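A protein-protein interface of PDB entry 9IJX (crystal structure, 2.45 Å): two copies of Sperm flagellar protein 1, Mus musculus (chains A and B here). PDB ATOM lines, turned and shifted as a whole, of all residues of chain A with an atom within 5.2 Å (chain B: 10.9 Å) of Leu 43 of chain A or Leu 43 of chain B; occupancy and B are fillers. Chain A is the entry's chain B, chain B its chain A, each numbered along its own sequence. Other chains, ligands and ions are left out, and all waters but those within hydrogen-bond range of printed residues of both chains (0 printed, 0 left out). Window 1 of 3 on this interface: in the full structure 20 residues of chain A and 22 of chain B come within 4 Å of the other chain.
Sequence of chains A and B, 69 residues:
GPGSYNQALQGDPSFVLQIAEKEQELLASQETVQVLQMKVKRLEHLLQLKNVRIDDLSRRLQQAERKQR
Of the 17 printed residues of chain B, 5 touch a printed residue of chain A. Hydrophobic or aromatic side chains of chain B that line the printed part of chain A: Val 40, Leu 43, Leu 46 and Leu 47. Of the 10 printed residues of chain A, 4 touch a printed residue of chain B. Among the printed residues, 8 pairs touch across the chains.
Lys 39 of chain A touches none of the printed residues of chain B. Printed residues of chain B within 4 Å of Val 40 of chain A: Lys 39 (3.9 Å) and Val 40 (3.7 Å). No residue of chain B comes within 4 Å of Arg 42 of chain A. Of the printed residues of chain B, Leu 43 of chain A touches Val 40 and Leu 43. No residue of chain B comes within 4 Å of Leu 46 of chain A. Of chain B, only Leu 43, Leu 46 and Leu 47 come within 4 Å of Leu 47 of chain A. Of the printed residues of chain A, Lys 39 of chain B touches Val 40 (3.9 Å). Glu 44 of chain B touches none of the printed residues of chain A. Printed residues of chain A within 4 Å of Leu 47 of chain B: Leu 47 (3.7 Å). The nearest residue of chain A that does not touch Leu 43 of chain B is Val 40 of chain A (4.6 Å).
Val 40 of chain A touches Lys 39 of chain B, but with the chains exchanged Lys 39 of chain A does not touch Val 40 of chain B (4.6 Å). Glu 44 of chain A touches Leu 43 of chain B, but with the chains exchanged Leu 43 of chain A does not touch Glu 44 of chain B (4.1 Å). Leu 47 of chain A touches Leu 46 of chain B, but with the chains exchanged Leu 46 of chain A does not touch Leu 47 of chain B (4.1 Å). Leu 47 of chain A touches its own counterpart, Leu 47 of chain B. Positions printed for both chains: 38, 39, 40, 41, 42, 43, 44, 45, 46 and 47.
Lys 39 of chain B touches Val 40 of chain A. CG2 of Val 40 of chain A touches CG2 of Val 40 of chain B (3.7 Å). Val 40 of chain B touches Leu 43 of chain A (O to CD1, 3.7 Å). CB of Leu 43 of chain B touches CD1 of Leu 43 of chain A, 3.5 Å away. Leu 43 of chain B touches Glu 44 of chain A. CD1 of Leu 47 of chain A touches CD1 of Leu 43 of chain B, 3.95 Å away. Leu 47 of chain A touches Leu 46 of chain B (CD1 to CB, 3.9 Å). Leu 47 of chain B touches Leu 47 of chain A (CD1 to CD2, 3.7 Å).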
ATOM      1  N   MET A  38     -21.054  16.598   2.663  1.00  0.00           N
ATOM      2  CA  MET A  38     -19.829  16.733   1.828  1.00  0.00           C
ATOM      3  C   MET A  38     -19.577  18.214   1.508  1.00  0.00           C
ATOM      4  O   MET A  38     -18.393  18.590   1.471  1.00  0.00           O
ATOM      5  CB  MET A  38     -19.931  15.929   0.526  1.00  0.00           C
ATOM      6  CG  MET A  38     -19.237  14.569   0.530  1.00  0.00           C
ATOM      7  SD  MET A  38     -18.461  14.028   2.077  1.00  0.00           S
ATOM      8  CE  MET A  38     -16.964  13.320   1.391  1.00  0.00           C
ATOM      9  N   LYS A  39     -20.634  19.004   1.289  1.00  0.00           N
ATOM     10  CA  LYS A  39     -20.531  20.470   1.056  1.00  0.00           C
ATOM     11  C   LYS A  39     -19.926  21.150   2.301  1.00  0.00           C
ATOM     12  O   LYS A  39     -18.971  21.946   2.140  1.00  0.00           O
ATOM     13  CB  LYS A  39     -21.897  21.056   0.682  1.00  0.00           C
ATOM     14  CG  LYS A  39     -22.444  20.648  -0.681  1.00  0.00           C
ATOM     15  CD  LYS A  39     -21.450  20.767  -1.832  1.00  0.00           C
ATOM     16  CE  LYS A  39     -22.100  20.626  -3.192  1.00  0.00           C
ATOM     17  NZ  LYS A  39     -21.283  21.237  -4.272  1.00  0.00           N
ATOM     18  N   VAL A  40     -20.445  20.835   3.493  1.00  0.00           N
ATOM     19  CA  VAL A  40     -19.911  21.335   4.797  1.00  0.00           C
ATOM     20  C   VAL A  40     -18.419  20.977   4.898  1.00  0.00           C
ATOM     21  O   VAL A  40     -17.620  21.870   5.257  1.00  0.00           O
ATOM     22  CB  VAL A  40     -20.723  20.786   5.989  1.00  0.00           C
ATOM     23  CG1 VAL A  40     -19.975  20.884   7.315  1.00  0.00           C
ATOM     24  CG2 VAL A  40     -22.077  21.464   6.089  1.00  0.00           C
ATOM     25  N   LYS A  41     -18.052  19.733   4.573  1.00  0.00           N
ATOM     26  CA  LYS A  41     -16.646  19.238   4.647  1.00  0.00           C
ATOM     27  C   LYS A  41     -15.760  20.070   3.715  1.00  0.00           C
ATOM     28  O   LYS A  41     -14.621  20.399   4.125  1.00  0.00           O
ATOM     29  CB  LYS A  41     -16.544  17.747   4.296  1.00  0.00           C
ATOM     30  CG  LYS A  41     -16.103  16.826   5.434  1.00  0.00           C
ATOM     31  CD  LYS A  41     -16.875  17.031   6.737  1.00  0.00           C
ATOM     32  CE  LYS A  41     -16.111  16.617   7.977  1.00  0.00           C
ATOM     33  NZ  LYS A  41     -15.907  15.150   8.034  1.00  0.00           N
ATOM     34  N   ARG A  42     -16.253  20.405   2.517  1.00  0.00           N
ATOM     35  CA  ARG A  42     -15.481  21.192   1.526  1.00  0.00           C
ATOM     36  C   ARG A  42     -15.352  22.632   2.032  1.00  0.00           C
ATOM     37  O   ARG A  42     -14.254  23.186   1.938  1.00  0.00           O
ATOM     38  CB  ARG A  42     -16.132  21.111   0.143  1.00  0.00           C
ATOM     39  CG  ARG A  42     -16.218  22.444  -0.574  1.00  0.00           C
ATOM     40  CD  ARG A  42     -16.923  22.294  -1.926  1.00  0.00           C
ATOM     41  NE  ARG A  42     -17.314  23.585  -2.480  1.00  0.00           N
ATOM     42  CZ  ARG A  42     -18.413  24.272  -2.153  1.00  0.00           C
ATOM     43  NH1 ARG A  42     -19.282  23.802  -1.268  1.00  0.00           N
ATOM     44  NH2 ARG A  42     -18.643  25.444  -2.726  1.00  0.00           N
ATOM     45  N   LEU A  43     -16.432  23.212   2.550  1.00  0.00           N
ATOM     46  CA  LEU A  43     -16.424  24.578   3.144  1.00  0.00           C
ATOM     47  C   LEU A  43     -15.401  24.627   4.291  1.00  0.00           C
ATOM     48  O   LEU A  43     -14.647  25.617   4.361  1.00  0.00           O
ATOM     49  CB  LEU A  43     -17.833  24.958   3.612  1.00  0.00           C
ATOM     50  CG  LEU A  43     -18.791  25.486   2.532  1.00  0.00           C
ATOM     51  CD1 LEU A  43     -20.063  26.041   3.163  1.00  0.00           C
ATOM     52  CD2 LEU A  43     -18.148  26.551   1.643  1.00  0.00           C
ATOM     53  N   GLU A  44     -15.337  23.591   5.126  1.00  0.00           N
ATOM     54  CA  GLU A  44     -14.376  23.505   6.264  1.00  0.00           C
ATOM     55  C   GLU A  44     -12.926  23.479   5.749  1.00  0.00           C
ATOM     56  O   GLU A  44     -12.049  24.121   6.385  1.00  0.00           O
ATOM     57  CB  GLU A  44     -14.691  22.298   7.147  1.00  0.00           C
ATOM     58  CG  GLU A  44     -16.042  22.424   7.851  1.00  0.00           C
ATOM     59  CD  GLU A  44     -16.218  21.812   9.234  1.00  0.00           C
ATOM     60  OE1 GLU A  44     -17.312  21.242   9.503  1.00  0.00           O
ATOM     61  OE2 GLU A  44     -15.281  21.946  10.053  1.00  0.00           O
ATOM     62  N   HIS A  45     -12.662  22.791   4.636  1.00  0.00           N
ATOM     63  CA  HIS A  45     -11.319  22.747   3.992  1.00  0.00           C
ATOM     64  C   HIS A  45     -10.954  24.147   3.476  1.00  0.00           C
ATOM     65  O   HIS A  45      -9.814  24.586   3.706  1.00  0.00           O
ATOM     66  CB  HIS A  45     -11.257  21.701   2.870  1.00  0.00           C
ATOM     67  CG  HIS A  45     -10.863  20.331   3.308  1.00  0.00           C
ATOM     68  ND1 HIS A  45     -11.783  19.426   3.809  1.00  0.00           N
ATOM     69  CD2 HIS A  45      -9.676  19.683   3.268  1.00  0.00           C
ATOM     70  CE1 HIS A  45     -11.177  18.284   4.076  1.00  0.00           C
ATOM     71  NE2 HIS A  45      -9.885  18.418   3.753  1.00  0.00           N
ATOM     72  N   LEU A  46     -11.884  24.809   2.786  1.00  0.00           N
ATOM     73  CA  LEU A  46     -11.749  26.216   2.310  1.00  0.00           C
ATOM     74  C   LEU A  46     -11.314  27.099   3.476  1.00  0.00           C
ATOM     75  O   LEU A  46     -10.338  27.838   3.310  1.00  0.00           O
ATOM     76  CB  LEU A  46     -13.082  26.725   1.749  1.00  0.00           C
ATOM     77  CG  LEU A  46     -13.166  26.812   0.226  1.00  0.00           C
ATOM     78  CD1 LEU A  46     -14.613  26.898  -0.247  1.00  0.00           C
ATOM     79  CD2 LEU A  46     -12.339  27.977  -0.275  1.00  0.00           C
ATOM     80  N   LEU A  47     -12.025  27.033   4.602  1.00  0.00           N
ATOM     81  CA  LEU A  47     -11.750  27.881   5.792  1.00  0.00           C
ATOM     82  C   LEU A  47     -10.301  27.672   6.238  1.00  0.00           C
ATOM     83  O   LEU A  47      -9.604  28.679   6.494  1.00  0.00           O
ATOM     84  CB  LEU A  47     -12.724  27.526   6.918  1.00  0.00           C
ATOM     85  CG  LEU A  47     -14.175  27.984   6.765  1.00  0.00           C
ATOM     86  CD1 LEU A  47     -14.810  28.162   8.139  1.00  0.00           C
ATOM     87  CD2 LEU A  47     -14.304  29.273   5.964  1.00  0.00           C
ATOM     88  N   VAL B  35     -31.046  21.704   9.116  1.00  0.00           N
ATOM     89  CA  VAL B  35     -29.946  22.175  10.022  1.00  0.00           C
ATOM     90  C   VAL B  35     -28.649  22.247   9.220  1.00  0.00           C
ATOM     91  O   VAL B  35     -27.881  23.180   9.457  1.00  0.00           O
ATOM     92  CB  VAL B  35     -29.748  21.314  11.294  1.00  0.00           C
ATOM     93  CG1 VAL B  35     -31.060  20.879  11.933  1.00  0.00           C
ATOM     94  CG2 VAL B  35     -28.819  20.121  11.078  1.00  0.00           C
ATOM     95  N   LEU B  36     -28.392  21.273   8.342  1.00  0.00           N
ATOM     96  CA  LEU B  36     -27.208  21.274   7.440  1.00  0.00           C
ATOM     97  C   LEU B  36     -27.283  22.517   6.544  1.00  0.00           C
ATOM     98  O   LEU B  36     -26.229  23.141   6.341  1.00  0.00           O
ATOM     99  CB  LEU B  36     -27.178  19.976   6.620  1.00  0.00           C
ATOM    100  CG  LEU B  36     -26.502  18.756   7.255  1.00  0.00           C
ATOM    101  CD1 LEU B  36     -24.997  18.947   7.342  1.00  0.00           C
ATOM    102  CD2 LEU B  36     -27.065  18.400   8.625  1.00  0.00           C
ATOM    103  N   GLN B  37     -28.476  22.893   6.079  1.00  0.00           N
ATOM    104  CA  GLN B  37     -28.694  24.085   5.213  1.00  0.00           C
ATOM    105  C   GLN B  37     -28.305  25.364   5.976  1.00  0.00           C
ATOM    106  O   GLN B  37     -27.755  26.302   5.339  1.00  0.00           O
ATOM    107  CB  GLN B  37     -30.141  24.144   4.725  1.00  0.00           C
ATOM    108  CG  GLN B  37     -30.470  23.106   3.659  1.00  0.00           C
ATOM    109  CD  GLN B  37     -31.953  22.927   3.424  1.00  0.00           C
ATOM    110  OE1 GLN B  37     -32.786  23.511   4.112  1.00  0.00           O
ATOM    111  NE2 GLN B  37     -32.290  22.107   2.441  1.00  0.00           N
ATOM    112  N   MET B  38     -28.579  25.413   7.283  1.00  0.00           N
ATOM    113  CA  MET B  38     -28.238  26.562   8.168  1.00  0.00           C
ATOM    114  C   MET B  38     -26.737  26.544   8.500  1.00  0.00           C
ATOM    115  O   MET B  38     -26.147  27.635   8.601  1.00  0.00           O
ATOM    116  CB  MET B  38     -29.042  26.530   9.474  1.00  0.00           C
ATOM    117  CG  MET B  38     -30.456  27.031   9.364  1.00  0.00           C
ATOM    118  SD  MET B  38     -31.137  27.474  10.997  1.00  0.00           S
ATOM    119  CE  MET B  38     -30.831  25.974  11.934  1.00  0.00           C
ATOM    120  N   LYS B  39     -26.139  25.359   8.668  1.00  0.00           N
ATOM    121  CA  LYS B  39     -24.680  25.178   8.915  1.00  0.00           C
ATOM    122  C   LYS B  39     -23.900  25.699   7.702  1.00  0.00           C
ATOM    123  O   LYS B  39     -22.951  26.472   7.914  1.00  0.00           O
ATOM    124  CB  LYS B  39     -24.352  23.710   9.232  1.00  0.00           C
ATOM    125  CG  LYS B  39     -22.871  23.375   9.388  1.00  0.00           C
ATOM    126  CD  LYS B  39     -22.484  22.538  10.594  1.00  0.00           C
ATOM    127  CE  LYS B  39     -20.984  22.552  10.805  1.00  0.00           C
ATOM    128  NZ  LYS B  39     -20.590  21.980  12.115  1.00  0.00           N
ATOM    129  N   VAL B  40     -24.293  25.310   6.484  1.00  0.00           N
ATOM    130  CA  VAL B  40     -23.688  25.805   5.208  1.00  0.00           C
ATOM    131  C   VAL B  40     -23.770  27.337   5.187  1.00  0.00           C
ATOM    132  O   VAL B  40     -22.743  27.965   4.873  1.00  0.00           O
ATOM    133  CB  VAL B  40     -24.360  25.160   3.980  1.00  0.00           C
ATOM    134  CG1 VAL B  40     -24.143  25.944   2.697  1.00  0.00           C
ATOM    135  CG2 VAL B  40     -23.906  23.720   3.814  1.00  0.00           C
ATOM    136  N   LYS B  41     -24.924  27.916   5.528  1.00  0.00           N
ATOM    137  CA  LYS B  41     -25.138  29.389   5.534  1.00  0.00           C
ATOM    138  C   LYS B  41     -24.158  30.055   6.516  1.00  0.00           C
ATOM    139  O   LYS B  41     -23.609  31.126   6.178  1.00  0.00           O
ATOM    140  CB  LYS B  41     -26.586  29.749   5.888  1.00  0.00           C
ATOM    141  CG  LYS B  41     -27.623  29.567   4.782  1.00  0.00           C
ATOM    142  CD  LYS B  41     -28.413  30.846   4.478  1.00  0.00           C
ATOM    143  CE  LYS B  41     -27.565  31.886   3.766  1.00  0.00           C
ATOM    144  NZ  LYS B  41     -27.971  33.280   4.078  1.00  0.00           N
ATOM    145  N   ARG B  42     -23.937  29.445   7.678  1.00  0.00           N
ATOM    146  CA  ARG B  42     -23.025  29.992   8.722  1.00  0.00           C
ATOM    147  C   ARG B  42     -21.577  29.874   8.220  1.00  0.00           C
ATOM    148  O   ARG B  42     -20.811  30.845   8.367  1.00  0.00           O
ATOM    149  CB  ARG B  42     -23.230  29.302  10.079  1.00  0.00           C
ATOM    150  CG  ARG B  42     -23.883  30.189  11.148  1.00  0.00           C
ATOM    151  CD  ARG B  42     -24.661  29.491  12.265  1.00  0.00           C
ATOM    152  NE  ARG B  42     -26.040  29.964  12.467  1.00  0.00           N
ATOM    153  CZ  ARG B  42     -26.718  29.935  13.616  1.00  0.00           C
ATOM    154  NH1 ARG B  42     -26.157  29.486  14.726  1.00  0.00           N
ATOM    155  NH2 ARG B  42     -27.962  30.378  13.652  1.00  0.00           N
ATOM    156  N   LEU B  43     -21.213  28.723   7.648  1.00  0.00           N
ATOM    157  CA  LEU B  43     -19.866  28.485   7.060  1.00  0.00           C
ATOM    158  C   LEU B  43     -19.606  29.534   5.974  1.00  0.00           C
ATOM    159  O   LEU B  43     -18.487  30.079   5.953  1.00  0.00           O
ATOM    160  CB  LEU B  43     -19.787  27.057   6.499  1.00  0.00           C
ATOM    161  CG  LEU B  43     -19.446  25.929   7.477  1.00  0.00           C
ATOM    162  CD1 LEU B  43     -17.941  25.799   7.634  1.00  0.00           C
ATOM    163  CD2 LEU B  43     -20.101  26.082   8.848  1.00  0.00           C
ATOM    164  N   GLU B  44     -20.605  29.832   5.131  1.00  0.00           N
ATOM    165  CA  GLU B  44     -20.495  30.835   4.035  1.00  0.00           C
ATOM    166  C   GLU B  44     -20.235  32.231   4.617  1.00  0.00           C
ATOM    167  O   GLU B  44     -19.437  32.962   4.005  1.00  0.00           O
ATOM    168  CB  GLU B  44     -21.751  30.836   3.164  1.00  0.00           C
ATOM    169  CG  GLU B  44     -21.920  29.571   2.351  1.00  0.00           C
ATOM    170  CD  GLU B  44     -23.279  29.407   1.684  1.00  0.00           C
ATOM    171  OE1 GLU B  44     -24.132  30.334   1.779  1.00  0.00           O
ATOM    172  OE2 GLU B  44     -23.503  28.328   1.087  1.00  0.00           O
ATOM    173  N   HIS B  45     -20.867  32.588   5.742  1.00  0.00           N
ATOM    174  CA  HIS B  45     -20.650  33.886   6.434  1.00  0.00           C
ATOM    175  C   HIS B  45     -19.208  33.958   6.944  1.00  0.00           C
ATOM    176  O   HIS B  45     -18.562  35.004   6.705  1.00  0.00           O
ATOM    177  CB  HIS B  45     -21.664  34.108   7.570  1.00  0.00           C
ATOM    178  CG  HIS B  45     -22.923  34.791   7.153  1.00  0.00           C
ATOM    179  ND1 HIS B  45     -24.139  34.539   7.765  1.00  0.00           N
ATOM    180  CD2 HIS B  45     -23.161  35.719   6.199  1.00  0.00           C
ATOM    181  CE1 HIS B  45     -25.072  35.284   7.202  1.00  0.00           C
ATOM    182  NE2 HIS B  45     -24.497  36.019   6.237  1.00  0.00           N
ATOM    183  N   LEU B  46     -18.741  32.895   7.615  1.00  0.00           N
ATOM    184  CA  LEU B  46     -17.338  32.753   8.081  1.00  0.00           C
ATOM    185  C   LEU B  46     -16.382  33.060   6.922  1.00  0.00           C
ATOM    186  O   LEU B  46     -15.467  33.894   7.101  1.00  0.00           O
ATOM    187  CB  LEU B  46     -17.081  31.328   8.581  1.00  0.00           C
ATOM    188  CG  LEU B  46     -16.875  31.170  10.083  1.00  0.00           C
ATOM    189  CD1 LEU B  46     -15.915  32.219  10.636  1.00  0.00           C
ATOM    190  CD2 LEU B  46     -18.218  31.230  10.770  1.00  0.00           C
ATOM    191  N   LEU B  47     -16.579  32.378   5.787  1.00  0.00           N
ATOM    192  CA  LEU B  47     -15.689  32.487   4.604  1.00  0.00           C
ATOM    193  C   LEU B  47     -15.613  33.951   4.170  1.00  0.00           C
ATOM    194  O   LEU B  47     -14.487  34.446   3.938  1.00  0.00           O
ATOM    195  CB  LEU B  47     -16.227  31.611   3.472  1.00  0.00           C
ATOM    196  CG  LEU B  47     -15.330  31.529   2.241  1.00  0.00           C
ATOM    197  CD1 LEU B  47     -14.116  30.659   2.527  1.00  0.00           C
ATOM    198  CD2 LEU B  47     -16.108  31.005   1.039  1.00  0.00           C
ATOM    199  N   GLN B  48     -16.769  34.618   4.082  1.00  0.00           N
ATOM    200  CA  GLN B  48     -16.852  36.052   3.707  1.00  0.00           C
ATOM    201  C   GLN B  48     -16.055  36.876   4.712  1.00  0.00           C
ATOM    202  O   GLN B  48     -15.292  37.739   4.265  1.00  0.00           O
ATOM    203  CB  GLN B  48     -18.303  36.527   3.600  1.00  0.00           C
ATOM    204  CG  GLN B  48     -18.513  37.592   2.523  1.00  0.00           C
ATOM    205  CD  GLN B  48     -17.634  37.442   1.298  1.00  0.00           C
ATOM    206  OE1 GLN B  48     -16.899  36.463   1.135  1.00  0.00           O
ATOM    207  NE2 GLN B  48     -17.692  38.435   0.426  1.00  0.00           N
ATOM    208  N   LEU B  49     -16.205  36.595   6.009  1.00  0.00           N
ATOM    209  CA  LEU B  49     -15.438  37.267   7.096  1.00  0.00           C
ATOM    210  C   LEU B  49     -13.937  37.050   6.867  1.00  0.00           C
ATOM    211  O   LEU B  49     -13.183  38.031   6.995  1.00  0.00           O
ATOM    212  CB  LEU B  49     -15.891  36.731   8.458  1.00  0.00           C
ATOM    213  CG  LEU B  49     -16.905  37.603   9.205  1.00  0.00           C
ATOM    214  CD1 LEU B  49     -18.064  38.007   8.307  1.00  0.00           C
ATOM    215  CD2 LEU B  49     -17.423  36.905  10.455  1.00  0.00           C
ATOM    216  N   LYS B  50     -13.528  35.829   6.508  1.00  0.00           N
ATOM    217  CA  LYS B  50     -12.097  35.491   6.278  1.00  0.00           C
ATOM    218  C   LYS B  50     -11.584  36.227   5.036  1.00  0.00           C
ATOM    219  O   LYS B  50     -10.432  36.691   5.053  1.00  0.00           O
ATOM    220  CB  LYS B  50     -11.911  33.978   6.138  1.00  0.00           C
ATOM    221  CG  LYS B  50     -12.349  33.178   7.364  1.00  0.00           C
ATOM    222  CD  LYS B  50     -11.396  32.080   7.779  1.00  0.00           C
ATOM    223  CE  LYS B  50     -11.227  31.970   9.281  1.00  0.00           C
ATOM    224  N   ASN B  51     -12.406  36.343   3.996  1.00  0.00           N
ATOM    225  CA  ASN B  51     -12.028  37.056   2.746  1.00  0.00           C
ATOM    226  C   ASN B  51     -11.785  38.540   3.043  1.00  0.00           C
ATOM    227  O   ASN B  51     -10.850  39.122   2.446  1.00  0.00           O
ATOM    228  CB  ASN B  51     -13.060  36.822   1.650  1.00  0.00           C
ATOM    229  CG  ASN B  51     -12.893  35.447   1.031  1.00  0.00           C
ATOM    230  OD1 ASN B  51     -11.823  34.847   1.111  1.00  0.00           O
ATOM    231  ND2 ASN B  51     -13.941  34.931   0.412  1.00  0.00           N
